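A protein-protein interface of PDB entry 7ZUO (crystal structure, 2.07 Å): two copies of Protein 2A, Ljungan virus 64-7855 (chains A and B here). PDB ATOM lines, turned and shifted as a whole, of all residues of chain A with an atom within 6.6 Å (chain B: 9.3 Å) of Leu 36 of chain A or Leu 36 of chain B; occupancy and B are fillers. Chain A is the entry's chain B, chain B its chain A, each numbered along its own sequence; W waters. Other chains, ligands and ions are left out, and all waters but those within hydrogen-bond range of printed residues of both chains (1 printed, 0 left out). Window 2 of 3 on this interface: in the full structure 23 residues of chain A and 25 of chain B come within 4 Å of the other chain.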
ATOM      1  N   PHE A  15      27.754 -17.018 -10.067  1.00  0.00           N
ATOM      2  CA  PHE A  15      27.786 -16.194  -8.868  1.00  0.00           C
ATOM      3  C   PHE A  15      28.038 -14.743  -9.292  1.00  0.00           C
ATOM      4  O   PHE A  15      27.526 -13.809  -8.673  1.00  0.00           O
ATOM      5  CB  PHE A  15      28.871 -16.700  -7.902  1.00  0.00           C
ATOM      6  CG  PHE A  15      29.152 -15.800  -6.731  1.00  0.00           C
ATOM      7  CD1 PHE A  15      28.176 -15.568  -5.774  1.00  0.00           C
ATOM      8  CD2 PHE A  15      30.387 -15.200  -6.565  1.00  0.00           C
ATOM      9  CE1 PHE A  15      28.416 -14.731  -4.685  1.00  0.00           C
ATOM     10  CE2 PHE A  15      30.635 -14.357  -5.493  1.00  0.00           C
ATOM     11  CZ  PHE A  15      29.651 -14.122  -4.552  1.00  0.00           C
ATOM     12  N   TYR A  16      28.902 -14.571 -10.300  1.00  0.00           N
ATOM     13  CA  TYR A  16      29.355 -13.246 -10.682  1.00  0.00           C
ATOM     14  C   TYR A  16      29.783 -13.254 -12.145  1.00  0.00           C
ATOM     15  O   TYR A  16      29.929 -14.324 -12.733  1.00  0.00           O
ATOM     16  CB  TYR A  16      30.515 -12.758  -9.807  1.00  0.00           C
ATOM     17  CG  TYR A  16      31.883 -13.325 -10.109  1.00  0.00           C
ATOM     18  CD1 TYR A  16      32.169 -14.673  -9.914  1.00  0.00           C
ATOM     19  CD2 TYR A  16      32.894 -12.517 -10.615  1.00  0.00           C
ATOM     20  CE1 TYR A  16      33.423 -15.188 -10.192  1.00  0.00           C
ATOM     21  CE2 TYR A  16      34.152 -13.016 -10.914  1.00  0.00           C
ATOM     22  CZ  TYR A  16      34.422 -14.362 -10.690  1.00  0.00           C
ATOM     23  OH  TYR A  16      35.683 -14.849 -10.965  1.00  0.00           O
ATOM     24  N   SER A  32      41.591 -15.845 -11.055  1.00  0.00           N
ATOM     25  CA  SER A  32      40.784 -16.033  -9.859  1.00  0.00           C
ATOM     26  C   SER A  32      39.404 -16.539 -10.250  1.00  0.00           C
ATOM     27  O   SER A  32      38.736 -15.895 -11.057  1.00  0.00           O
ATOM     28  CB  SER A  32      40.672 -14.738  -9.092  1.00  0.00           C
ATOM     29  OG  SER A  32      39.340 -14.542  -8.622  1.00  0.00           O
ATOM     30  N   ASP A  34      36.780 -17.058  -8.057  1.00  0.00           N
ATOM     31  CA  ASP A  34      35.701 -16.637  -7.172  1.00  0.00           C
ATOM     32  C   ASP A  34      36.010 -15.239  -6.651  1.00  0.00           C
ATOM     33  O   ASP A  34      36.964 -15.060  -5.908  1.00  0.00           O
ATOM     34  CB  ASP A  34      35.502 -17.661  -6.040  1.00  0.00           C
ATOM     35  CG  ASP A  34      34.266 -17.399  -5.183  1.00  0.00           C
ATOM     36  OD1 ASP A  34      34.007 -16.206  -4.885  1.00  0.00           O
ATOM     37  OD2 ASP A  34      33.540 -18.381  -4.839  1.00  0.00           O
ATOM     38  N   ILE A  35      35.207 -14.236  -7.051  1.00  0.00           N
ATOM     39  CA  ILE A  35      35.518 -12.848  -6.727  1.00  0.00           C
ATOM     40  C   ILE A  35      35.477 -12.667  -5.200  1.00  0.00           C
ATOM     41  O   ILE A  35      36.153 -11.824  -4.664  1.00  0.00           O
ATOM     42  CB  ILE A  35      34.587 -11.857  -7.466  1.00  0.00           C
ATOM     43  CG1 ILE A  35      35.035 -10.399  -7.292  1.00  0.00           C
ATOM     44  CG2 ILE A  35      33.130 -12.001  -7.044  1.00  0.00           C
ATOM     45  CD1 ILE A  35      36.510 -10.166  -7.639  1.00  0.00           C
ATOM     46  N   LEU A  36      34.666 -13.441  -4.469  1.00  0.00           N
ATOM     47  CA  LEU A  36      34.615 -13.283  -3.027  1.00  0.00           C
ATOM     48  C   LEU A  36      35.958 -13.706  -2.408  1.00  0.00           C
ATOM     49  O   LEU A  36      36.517 -12.999  -1.573  1.00  0.00           O
ATOM     50  CB  LEU A  36      33.432 -14.060  -2.454  1.00  0.00           C
ATOM     51  CG  LEU A  36      33.343 -13.990  -0.937  1.00  0.00           C
ATOM     52  CD1 LEU A  36      33.285 -12.529  -0.452  1.00  0.00           C
ATOM     53  CD2 LEU A  36      32.193 -14.821  -0.411  1.00  0.00           C
ATOM     54  N   THR A  37      36.505 -14.824  -2.898  1.00  0.00           N
ATOM     55  CA  THR A  37      37.787 -15.326  -2.443  1.00  0.00           C
ATOM     56  C   THR A  37      38.896 -14.302  -2.704  1.00  0.00           C
ATOM     57  O   THR A  37      39.713 -14.004  -1.832  1.00  0.00           O
ATOM     58  CB  THR A  37      38.128 -16.647  -3.134  1.00  0.00           C
ATOM     59  OG1 THR A  37      37.053 -17.560  -2.907  1.00  0.00           O
ATOM     60  CG2 THR A  37      39.438 -17.198  -2.634  1.00  0.00           C
ATOM     61  N   THR A  38      38.898 -13.761  -3.920  1.00  0.00           N
ATOM     62  CA  THR A  38      39.900 -12.799  -4.357  1.00  0.00           C
ATOM     63  C   THR A  38      39.832 -11.545  -3.483  1.00  0.00           C
ATOM     64  O   THR A  38      40.853 -11.086  -2.980  1.00  0.00           O
ATOM     65  CB  THR A  38      39.716 -12.465  -5.851  1.00  0.00           C
ATOM     66  OG1 THR A  38      39.846 -13.699  -6.553  1.00  0.00           O
ATOM     67  CG2 THR A  38      40.758 -11.508  -6.404  1.00  0.00           C
ATOM     68  N   ALA A  39      38.630 -10.977  -3.339  1.00  0.00           N
ATOM     69  CA  ALA A  39      38.453  -9.795  -2.515  1.00  0.00           C
ATOM     70  C   ALA A  39      38.998 -10.022  -1.102  1.00  0.00           C
ATOM     71  O   ALA A  39      39.758  -9.192  -0.618  1.00  0.00           O
ATOM     72  CB  ALA A  39      37.011  -9.399  -2.492  1.00  0.00           C
ATOM     73  N   ILE A  40      38.612 -11.126  -0.445  1.00  0.00           N
ATOM     74  CA  ILE A  40      38.940 -11.335   0.956  1.00  0.00           C
ATOM     75  C   ILE A  40      40.404 -11.725   1.121  1.00  0.00           C
ATOM     76  O   ILE A  40      41.064 -11.222   2.028  1.00  0.00           O
ATOM     77  CB  ILE A  40      38.003 -12.368   1.603  1.00  0.00           C
ATOM     78  CG1 ILE A  40      36.574 -11.829   1.679  1.00  0.00           C
ATOM     79  CG2 ILE A  40      38.540 -12.806   2.959  1.00  0.00           C
ATOM     80  CD1 ILE A  40      36.472 -10.536   2.433  1.00  0.00           C
ATOM     81  N   THR A  41      40.927 -12.566   0.222  1.00  0.00           N
ATOM     82  CA  THR A  41      42.344 -12.921   0.232  1.00  0.00           C
ATOM     83  C   THR A  41      43.253 -11.705   0.008  1.00  0.00           C
ATOM     84  O   THR A  41      44.322 -11.620   0.598  1.00  0.00           O
ATOM     85  CB  THR A  41      42.638 -14.017  -0.788  1.00  0.00           C
ATOM     86  OG1 THR A  41      41.811 -15.128  -0.456  1.00  0.00           O
ATOM     87  CG2 THR A  41      44.078 -14.469  -0.764  1.00  0.00           C
ATOM     88  N   LEU A 119      32.895  -7.375  -8.639  1.00  0.00           N
ATOM     89  CA  LEU A 119      32.082  -7.305  -7.430  1.00  0.00           C
ATOM     90  C   LEU A 119      30.707  -6.697  -7.714  1.00  0.00           C
ATOM     91  O   LEU A 119      29.683  -7.227  -7.272  1.00  0.00           O
ATOM     92  CB  LEU A 119      32.813  -6.508  -6.333  1.00  0.00           C
ATOM     93  CG  LEU A 119      33.884  -7.312  -5.578  1.00  0.00           C
ATOM     94  CD1 LEU A 119      34.747  -6.429  -4.708  1.00  0.00           C
ATOM     95  CD2 LEU A 119      33.251  -8.406  -4.722  1.00  0.00           C
ATOM     96  N   LEU A 122      27.443  -8.503  -9.025  1.00  0.00           N
ATOM     97  CA  LEU A 122      26.458  -9.169  -8.189  1.00  0.00           C
ATOM     98  C   LEU A 122      25.105  -8.445  -8.190  1.00  0.00           C
ATOM     99  O   LEU A 122      24.102  -9.060  -7.853  1.00  0.00           O
ATOM    100  CB  LEU A 122      27.017  -9.309  -6.772  1.00  0.00           C
ATOM    101  CG  LEU A 122      27.767 -10.614  -6.526  1.00  0.00           C
ATOM    102  CD1 LEU A 122      29.108 -10.642  -7.236  1.00  0.00           C
ATOM    103  CD2 LEU A 122      27.951 -10.818  -5.043  1.00  0.00           C
ATOM    104  N   ARG B  13      29.269  -5.704   9.377  1.00  0.00           N
ATOM    105  CA  ARG B  13      28.412  -6.875   9.369  1.00  0.00           C
ATOM    106  C   ARG B  13      29.269  -8.029   8.848  1.00  0.00           C
ATOM    107  O   ARG B  13      29.598  -8.078   7.674  1.00  0.00           O
ATOM    108  CB  ARG B  13      27.157  -6.570   8.538  1.00  0.00           C
ATOM    109  CG  ARG B  13      25.931  -7.418   8.859  1.00  0.00           C
ATOM    110  CD  ARG B  13      24.655  -6.945   8.134  1.00  0.00           C
ATOM    111  NE  ARG B  13      24.025  -5.669   8.558  1.00  0.00           N
ATOM    112  CZ  ARG B  13      22.779  -5.528   9.044  1.00  0.00           C
ATOM    113  NH1 ARG B  13      22.160  -6.548   9.619  1.00  0.00           N
ATOM    114  NH2 ARG B  13      22.165  -4.355   9.004  1.00  0.00           N
ATOM    115  N   PHE B  15      32.207  -9.828   7.479  1.00  0.00           N
ATOM    116  CA  PHE B  15      33.424  -9.419   6.787  1.00  0.00           C
ATOM    117  C   PHE B  15      33.183  -8.306   5.765  1.00  0.00           C
ATOM    118  O   PHE B  15      34.056  -8.052   4.945  1.00  0.00           O
ATOM    119  CB  PHE B  15      34.178 -10.620   6.191  1.00  0.00           C
ATOM    120  CG  PHE B  15      33.416 -11.531   5.267  1.00  0.00           C
ATOM    121  CD1 PHE B  15      32.867 -11.063   4.094  1.00  0.00           C
ATOM    122  CD2 PHE B  15      33.295 -12.882   5.569  1.00  0.00           C
ATOM    123  CE1 PHE B  15      32.200 -11.923   3.238  1.00  0.00           C
ATOM    124  CE2 PHE B  15      32.619 -13.742   4.720  1.00  0.00           C
ATOM    125  CZ  PHE B  15      32.077 -13.266   3.549  1.00  0.00           C
ATOM    126  N   TYR B  16      32.041  -7.612   5.855  1.00  0.00           N
ATOM    127  CA  TYR B  16      31.778  -6.459   5.014  1.00  0.00           C
ATOM    128  C   TYR B  16      31.142  -5.344   5.844  1.00  0.00           C
ATOM    129  O   TYR B  16      30.937  -5.471   7.055  1.00  0.00           O
ATOM    130  CB  TYR B  16      30.918  -6.881   3.817  1.00  0.00           C
ATOM    131  CG  TYR B  16      29.511  -7.269   4.179  1.00  0.00           C
ATOM    132  CD1 TYR B  16      29.212  -8.560   4.586  1.00  0.00           C
ATOM    133  CD2 TYR B  16      28.484  -6.340   4.148  1.00  0.00           C
ATOM    134  CE1 TYR B  16      27.921  -8.919   4.937  1.00  0.00           C
ATOM    135  CE2 TYR B  16      27.185  -6.680   4.516  1.00  0.00           C
ATOM    136  CZ  TYR B  16      26.904  -7.980   4.913  1.00  0.00           C
ATOM    137  OH  TYR B  16      25.629  -8.368   5.259  1.00  0.00           O
ATOM    138  N   SER B  32      18.544  -5.143   4.910  1.00  0.00           N
ATOM    139  CA  SER B  32      19.249  -6.270   4.317  1.00  0.00           C
ATOM    140  C   SER B  32      20.085  -6.945   5.396  1.00  0.00           C
ATOM    141  O   SER B  32      20.984  -6.317   5.954  1.00  0.00           O
ATOM    142  CB  SER B  32      20.124  -5.799   3.165  1.00  0.00           C
ATOM    143  OG  SER B  32      21.059  -6.800   2.730  1.00  0.00           O
ATOM    144  N   GLN B  33      19.828  -8.228   5.646  1.00  0.00           N
ATOM    145  CA  GLN B  33      20.606  -8.985   6.624  1.00  0.00           C
ATOM    146  C   GLN B  33      21.963  -9.384   6.033  1.00  0.00           C
ATOM    147  O   GLN B  33      22.945  -9.530   6.761  1.00  0.00           O
ATOM    148  CB  GLN B  33      19.827 -10.213   7.130  1.00  0.00           C
ATOM    149  CG  GLN B  33      18.651  -9.880   8.052  1.00  0.00           C
ATOM    150  CD  GLN B  33      19.038  -9.075   9.277  1.00  0.00           C
ATOM    151  OE1 GLN B  33      18.592  -7.943   9.481  1.00  0.00           O
ATOM    152  NE2 GLN B  33      19.884  -9.655  10.114  1.00  0.00           N
ATOM    153  N   ASP B  34      22.020  -9.581   4.709  1.00  0.00           N
ATOM    154  CA  ASP B  34      23.196 -10.185   4.114  1.00  0.00           C
ATOM    155  C   ASP B  34      23.342  -9.708   2.676  1.00  0.00           C
ATOM    156  O   ASP B  34      22.430  -9.891   1.893  1.00  0.00           O
ATOM    157  CB  ASP B  34      23.125 -11.717   4.181  1.00  0.00           C
ATOM    158  CG  ASP B  34      24.292 -12.344   3.455  1.00  0.00           C
ATOM    159  OD1 ASP B  34      25.415 -12.087   3.892  1.00  0.00           O
ATOM    160  OD2 ASP B  34      24.074 -12.983   2.399  1.00  0.00           O
ATOM    161  N   ILE B  35      24.508  -9.142   2.351  1.00  0.00           N
ATOM    162  CA  ILE B  35      24.740  -8.493   1.068  1.00  0.00           C
ATOM    163  C   ILE B  35      24.642  -9.497  -0.079  1.00  0.00           C
ATOM    164  O   ILE B  35      24.024  -9.176  -1.089  1.00  0.00           O
ATOM    165  CB  ILE B  35      26.062  -7.676   1.048  1.00  0.00           C
ATOM    166  CG1 ILE B  35      26.202  -6.844  -0.239  1.00  0.00           C
ATOM    167  CG2 ILE B  35      27.297  -8.552   1.288  1.00  0.00           C
ATOM    168  CD1 ILE B  35      24.991  -5.954  -0.523  1.00  0.00           C
ATOM    169  N   LEU B  36      25.227 -10.708   0.035  1.00  0.00           N
ATOM    170  CA  LEU B  36      25.209 -11.618  -1.100  1.00  0.00           C
ATOM    171  C   LEU B  36      23.790 -12.124  -1.349  1.00  0.00           C
ATOM    172  O   LEU B  36      23.365 -12.258  -2.500  1.00  0.00           O
ATOM    173  CB  LEU B  36      26.164 -12.795  -0.897  1.00  0.00           C
ATOM    174  CG  LEU B  36      27.647 -12.467  -0.699  1.00  0.00           C
ATOM    175  CD1 LEU B  36      28.477 -13.744  -0.875  1.00  0.00           C
ATOM    176  CD2 LEU B  36      28.127 -11.381  -1.634  1.00  0.00           C
ATOM    177  N   THR B  37      23.076 -12.420  -0.258  1.00  0.00           N
ATOM    178  CA  THR B  37      21.688 -12.851  -0.331  1.00  0.00           C
ATOM    179  C   THR B  37      20.861 -11.749  -0.989  1.00  0.00           C
ATOM    180  O   THR B  37      20.095 -12.034  -1.908  1.00  0.00           O
ATOM    181  CB  THR B  37      21.132 -13.252   1.043  1.00  0.00           C
ATOM    182  OG1 THR B  37      21.956 -14.326   1.481  1.00  0.00           O
ATOM    183  CG2 THR B  37      19.690 -13.728   1.016  1.00  0.00           C
ATOM    184  N   THR B  38      21.034 -10.511  -0.506  1.00  0.00           N
ATOM    185  CA  THR B  38      20.287  -9.378  -1.029  1.00  0.00           C
ATOM    186  C   THR B  38      20.569  -9.248  -2.532  1.00  0.00           C
ATOM    187  O   THR B  38      19.654  -9.026  -3.333  1.00  0.00           O
ATOM    188  CB  THR B  38      20.569  -8.102  -0.216  1.00  0.00           C
ATOM    189  OG1 THR B  38      19.884  -8.230   1.032  1.00  0.00           O
ATOM    190  CG2 THR B  38      20.092  -6.823  -0.882  1.00  0.00           C
ATOM    191  N   ALA B  39      21.839  -9.381  -2.934  1.00  0.00           N
ATOM    192  CA  ALA B  39      22.202  -9.163  -4.324  1.00  0.00           C
ATOM    193  C   ALA B  39      21.489 -10.184  -5.211  1.00  0.00           C
ATOM    194  O   ALA B  39      20.921  -9.830  -6.255  1.00  0.00           O
ATOM    195  CB  ALA B  39      23.699  -9.227  -4.487  1.00  0.00           C
ATOM    196  N   ILE B  40      21.501 -11.447  -4.774  1.00  0.00           N
ATOM    197  CA  ILE B  40      20.973 -12.508  -5.605  1.00  0.00           C
ATOM    198  C   ILE B  40      19.446 -12.449  -5.596  1.00  0.00           C
ATOM    199  O   ILE B  40      18.842 -12.626  -6.646  1.00  0.00           O
ATOM    200  CB  ILE B  40      21.595 -13.881  -5.253  1.00  0.00           C
ATOM    201  CG1 ILE B  40      21.429 -14.869  -6.413  1.00  0.00           C
ATOM    202  CG2 ILE B  40      21.077 -14.450  -3.948  1.00  0.00           C
ATOM    203  CD1 ILE B  40      22.089 -16.202  -6.174  1.00  0.00           C
ATOM    204  N   THR B  41      18.852 -12.110  -4.448  1.00  0.00           N
ATOM    205  CA  THR B  41      17.415 -11.914  -4.323  1.00  0.00           C
ATOM    206  C   THR B  41      16.914 -10.785  -5.235  1.00  0.00           C
ATOM    207  O   THR B  41      15.826 -10.890  -5.802  1.00  0.00           O
ATOM    208  CB  THR B  41      17.063 -11.661  -2.850  1.00  0.00           C
ATOM    209  OG1 THR B  41      17.429 -12.838  -2.135  1.00  0.00           O
ATOM    210  CG2 THR B  41      15.597 -11.380  -2.609  1.00  0.00           C
ATOM    211  N   GLY B  42      17.680  -9.690  -5.360  1.00  0.00           N
ATOM    212  CA  GLY B  42      17.369  -8.670  -6.342  1.00  0.00           C
ATOM    213  C   GLY B  42      16.308  -7.665  -5.887  1.00  0.00           C
ATOM    214  O   GLY B  42      15.778  -6.903  -6.699  1.00  0.00           O
ATOM    215  N   LYS B  43      15.977  -7.641  -4.598  1.00  0.00           N
ATOM    216  CA  LYS B  43      15.147  -6.556  -4.113  1.00  0.00           C
ATOM    217  C   LYS B  43      15.403  -6.272  -2.640  1.00  0.00           C
ATOM    218  O   LYS B  43      15.897  -7.118  -1.911  1.00  0.00           O
ATOM    219  CB  LYS B  43      13.663  -6.786  -4.411  1.00  0.00           C
ATOM    220  CG  LYS B  43      13.076  -8.116  -3.973  1.00  0.00           C
ATOM    221  CD  LYS B  43      11.606  -8.209  -4.388  1.00  0.00           C
ATOM    222  CE  LYS B  43      11.261  -9.504  -5.095  1.00  0.00           C
ATOM    223  NZ  LYS B  43      11.222 -10.640  -4.140  1.00  0.00           N
ATOM    224  N   LYS B  78      19.807  -5.654 -11.639  1.00  0.00           N
ATOM    225  CA  LYS B  78      18.428  -6.116 -11.729  1.00  0.00           C
ATOM    226  C   LYS B  78      17.631  -5.640 -10.512  1.00  0.00           C
ATOM    227  O   LYS B  78      16.478  -6.050 -10.330  1.00  0.00           O
ATOM    228  CB  LYS B  78      18.410  -7.651 -11.833  1.00  0.00           C
ATOM    229  CG  LYS B  78      18.868  -8.354 -10.563  1.00  0.00           C
ATOM    230  CD  LYS B  78      18.873  -9.856 -10.628  1.00  0.00           C
ATOM    231  CE  LYS B  78      19.080 -10.380  -9.226  1.00  0.00           C
ATOM    232  NZ  LYS B  78      19.357 -11.818  -9.182  1.00  0.00           N
ATOM    233  N   HIS B  79      18.265  -4.845  -9.629  1.00  0.00           N
ATOM    234  CA  HIS B  79      17.717  -4.668  -8.293  1.00  0.00           C
ATOM    235  C   HIS B  79      16.502  -3.751  -8.329  1.00  0.00           C
ATOM    236  O   HIS B  79      16.443  -2.831  -9.124  1.00  0.00           O
ATOM    237  CB  HIS B  79      18.750  -4.095  -7.314  1.00  0.00           C
ATOM    238  CG  HIS B  79      18.605  -4.639  -5.928  1.00  0.00           C
ATOM    239  ND1 HIS B  79      19.217  -5.790  -5.491  1.00  0.00           N
ATOM    240  CD2 HIS B  79      17.885  -4.145  -4.888  1.00  0.00           C
ATOM    241  CE1 HIS B  79      18.882  -5.996  -4.222  1.00  0.00           C
ATOM    242  NE2 HIS B  79      18.053  -4.977  -3.815  1.00  0.00           N
ATOM    243  N   LEU B 115      24.259  -0.431  -1.987  1.00  0.00           N
ATOM    244  CA  LEU B 115      24.599  -1.827  -2.233  1.00  0.00           C
ATOM    245  C   LEU B 115      25.999  -1.896  -2.836  1.00  0.00           C
ATOM    246  O   LEU B 115      26.762  -2.803  -2.510  1.00  0.00           O
ATOM    247  CB  LEU B 115      23.610  -2.493  -3.191  1.00  0.00           C
ATOM    248  CG  LEU B 115      22.201  -2.798  -2.672  1.00  0.00           C
ATOM    249  CD1 LEU B 115      21.359  -3.436  -3.779  1.00  0.00           C
ATOM    250  CD2 LEU B 115      22.242  -3.727  -1.457  1.00  0.00           C
ATOM    251  N   SER B 118      28.592  -1.479  -0.118  1.00  0.00           N
ATOM    252  CA  SER B 118      28.675  -2.691   0.675  1.00  0.00           C
ATOM    253  C   SER B 118      29.484  -3.746  -0.070  1.00  0.00           C
ATOM    254  O   SER B 118      30.385  -4.385   0.498  1.00  0.00           O
ATOM    255  CB  SER B 118      27.297  -3.162   1.006  1.00  0.00           C
ATOM    256  OG  SER B 118      27.344  -4.180   1.964  1.00  0.00           O
ATOM    257  N   LEU B 119      29.172  -3.916  -1.367  1.00  0.00           N
ATOM    258  CA  LEU B 119      29.906  -4.878  -2.159  1.00  0.00           C
ATOM    259  C   LEU B 119      31.390  -4.513  -2.212  1.00  0.00           C
ATOM    260  O   LEU B 119      32.249  -5.389  -2.047  1.00  0.00           O
ATOM    261  CB  LEU B 119      29.309  -4.965  -3.563  1.00  0.00           C
ATOM    262  CG  LEU B 119      28.000  -5.721  -3.662  1.00  0.00           C
ATOM    263  CD1 LEU B 119      27.400  -5.546  -5.043  1.00  0.00           C
ATOM    264  CD2 LEU B 119      28.208  -7.204  -3.359  1.00  0.00           C
ATOM    265  N   LEU B 120      31.718  -3.233  -2.459  1.00  0.00           N
ATOM    266  CA  LEU B 120      33.123  -2.879  -2.608  1.00  0.00           C
ATOM    267  C   LEU B 120      33.852  -2.829  -1.250  1.00  0.00           C
ATOM    268  O   LEU B 120      35.072  -2.911  -1.238  1.00  0.00           O
ATOM    269  CB  LEU B 120      33.219  -1.577  -3.412  1.00  0.00           C
ATOM    270  CG  LEU B 120      32.791  -1.706  -4.874  1.00  0.00           C
ATOM    271  CD1 LEU B 120      32.990  -0.417  -5.632  1.00  0.00           C
ATOM    272  CD2 LEU B 120      33.554  -2.801  -5.568  1.00  0.00           C
ATOM    273  N   SER B 121      33.136  -2.834  -0.114  1.00  0.00           N
ATOM    274  CA  SER B 121      33.731  -3.011   1.216  1.00  0.00           C
ATOM    275  C   SER B 121      34.442  -4.361   1.381  1.00  0.00           C
ATOM    276  O   SER B 121      35.265  -4.543   2.307  1.00  0.00           O
ATOM    277  CB  SER B 121      32.682  -2.811   2.328  1.00  0.00           C
ATOM    278  OG  SER B 121      31.814  -3.947   2.492  1.00  0.00           O
ATOM    279  N   LEU B 122      34.153  -5.316   0.471  1.00  0.00           N
ATOM    280  CA  LEU B 122      34.870  -6.577   0.459  1.00  0.00           C
ATOM    281  C   LEU B 122      36.342  -6.413   0.060  1.00  0.00           C
ATOM    282  O   LEU B 122      37.148  -7.306   0.347  1.00  0.00           O
ATOM    283  CB  LEU B 122      34.138  -7.543  -0.475  1.00  0.00           C
ATOM    284  CG  LEU B 122      32.774  -8.044   0.013  1.00  0.00           C
ATOM    285  CD1 LEU B 122      32.044  -8.767  -1.117  1.00  0.00           C
ATOM    286  CD2 LEU B 122      32.953  -8.987   1.202  1.00  0.00           C
ATOM    287  N   LEU B 123      36.700  -5.261  -0.538  1.00  0.00           N
ATOM    288  CA  LEU B 123      38.089  -4.910  -0.836  1.00  0.00           C
ATOM    289  C   LEU B 123      38.789  -4.187   0.312  1.00  0.00           C
ATOM    290  O   LEU B 123      39.981  -3.890   0.203  1.00  0.00           O
ATOM    291  CB  LEU B 123      38.109  -3.982  -2.046  1.00  0.00           C
ATOM    292  CG  LEU B 123      37.574  -4.622  -3.321  1.00  0.00           C
ATOM    293  CD1 LEU B 123      37.631  -3.650  -4.485  1.00  0.00           C
ATOM    294  CD2 LEU B 123      38.334  -5.894  -3.622  1.00  0.00           C
HETATM  295  O   HOH W   1      39.313  -7.583   1.932  1.00  0.00           O
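The side-chain carboxylate (OD1) of Asp 34 of chain A lies within hydrogen-bond range of the backbone NH (N) of Leu 36 of chain A (2.9 Å). The backbone NH (N) of Leu 36 of chain B sits close to the side-chain carboxylate (OD2) of Asp 34 of chain B.
No residue of chain B comes within 4 Å of Ile 35 of chain A. Leu 36 of chain A touches just these residues of chain B: Phe 15, Leu 36 and Leu 122. No residue of chain B comes within 4 Å of Thr 37 of chain A. Thr 41 of chain B touches none of the printed residues of chain A. Of the printed residues of chain A, Leu 119 of chain B touches Leu 119 (3.6 Å) and Leu 122 (3.995 Å). Printed residues of chain A within 4 Å of Leu 123 of chain B: Ala 39 (3.9 Å) and Leu 119 (3.6 Å). The nearest printed residue of chain B that does not touch Leu 36 of chain A is Leu 119 of chain B (7.4 Å). The nearest printed residue of chain A that does not touch Leu 36 of chain B is Leu 119 of chain A (6.7 Å). The nearest printed residue of chain A that does not touch Leu 122 of chain B is Leu 122 of chain A (6.0 Å).
Among the printed residues, pairs that only touch across the chains: Leu 122 of chain A with Ala 39 of chain B (3.4 Å), Leu 122 of chain A with Leu 36 of chain B (3.5 Å), Leu 119 of chain A with Leu 119 of chain B (3.6 Å), Leu 119 of chain A with Leu 123 of chain B (3.6 Å), Leu 119 of chain A with Leu 122 of chain B (3.8 Å), Leu 119 of chain A with Leu 120 of chain B (3.9 Å), Phe 15 of chain A with Leu 36 of chain B (3.9 Å), Leu 36 of chain A with Phe 15 of chain B (3.9 Å), Leu 36 of chain A with Leu 36 of chain B (3.9 Å), Ile 40 of chain A with Leu 122 of chain B (3.9 Å), Ala 39 of chain A with Leu 123 of chain B (3.9 Å), Leu 36 of chain A with Leu 122 of chain B (3.9 Å) and Leu 122 of chain A with Leu 119 of chain B (3.995 Å).
O of Leu 122 of chain B lies close to O of Ala 39 of chain A (3.4 Å).
Leu 36 of chain A touches its own counterpart, Leu 36 of chain B. Leu 36 of chain A touches Leu 122 of chain B, and with the chains exchanged Leu 122 of chain A touches Leu 36 of chain B. Leu 119 of chain A touches its own counterpart, Leu 119 of chain B. Leu 119 of chain A touches Leu 122 of chain B, and with the chains exchanged Leu 122 of chain A touches Leu 119 of chain B. Positions printed for both chains: 15, 16, 32, 34, 35, 36, 37, 38, 39, 40, 41, 119 and 122.
Water W1 lies within hydrogen-bond range of O of Leu 122 of chain B and O of Ala 39 of chain A.
Of the 13 printed residues of chain A, 6 touch a printed residue of chain B. Printed residues of chain A that touch a printed residue of chain B: Phe 15, Leu 36, Ala 39, Ile 40, Leu 119 and Leu 122. Hydrophobic or aromatic side chains of chain A within 4 Å of the printed part of chain B: Phe 15, Leu 36, Ala 39, Ile 40, Leu 119 and Leu 122. Of the 24 printed residues of chain B, 7 touch a printed residue of chain A. Among the printed residues, no Asp or Glu carboxylate lies within 4 Å of a Lys or Arg side-chain nitrogen of the other chain.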
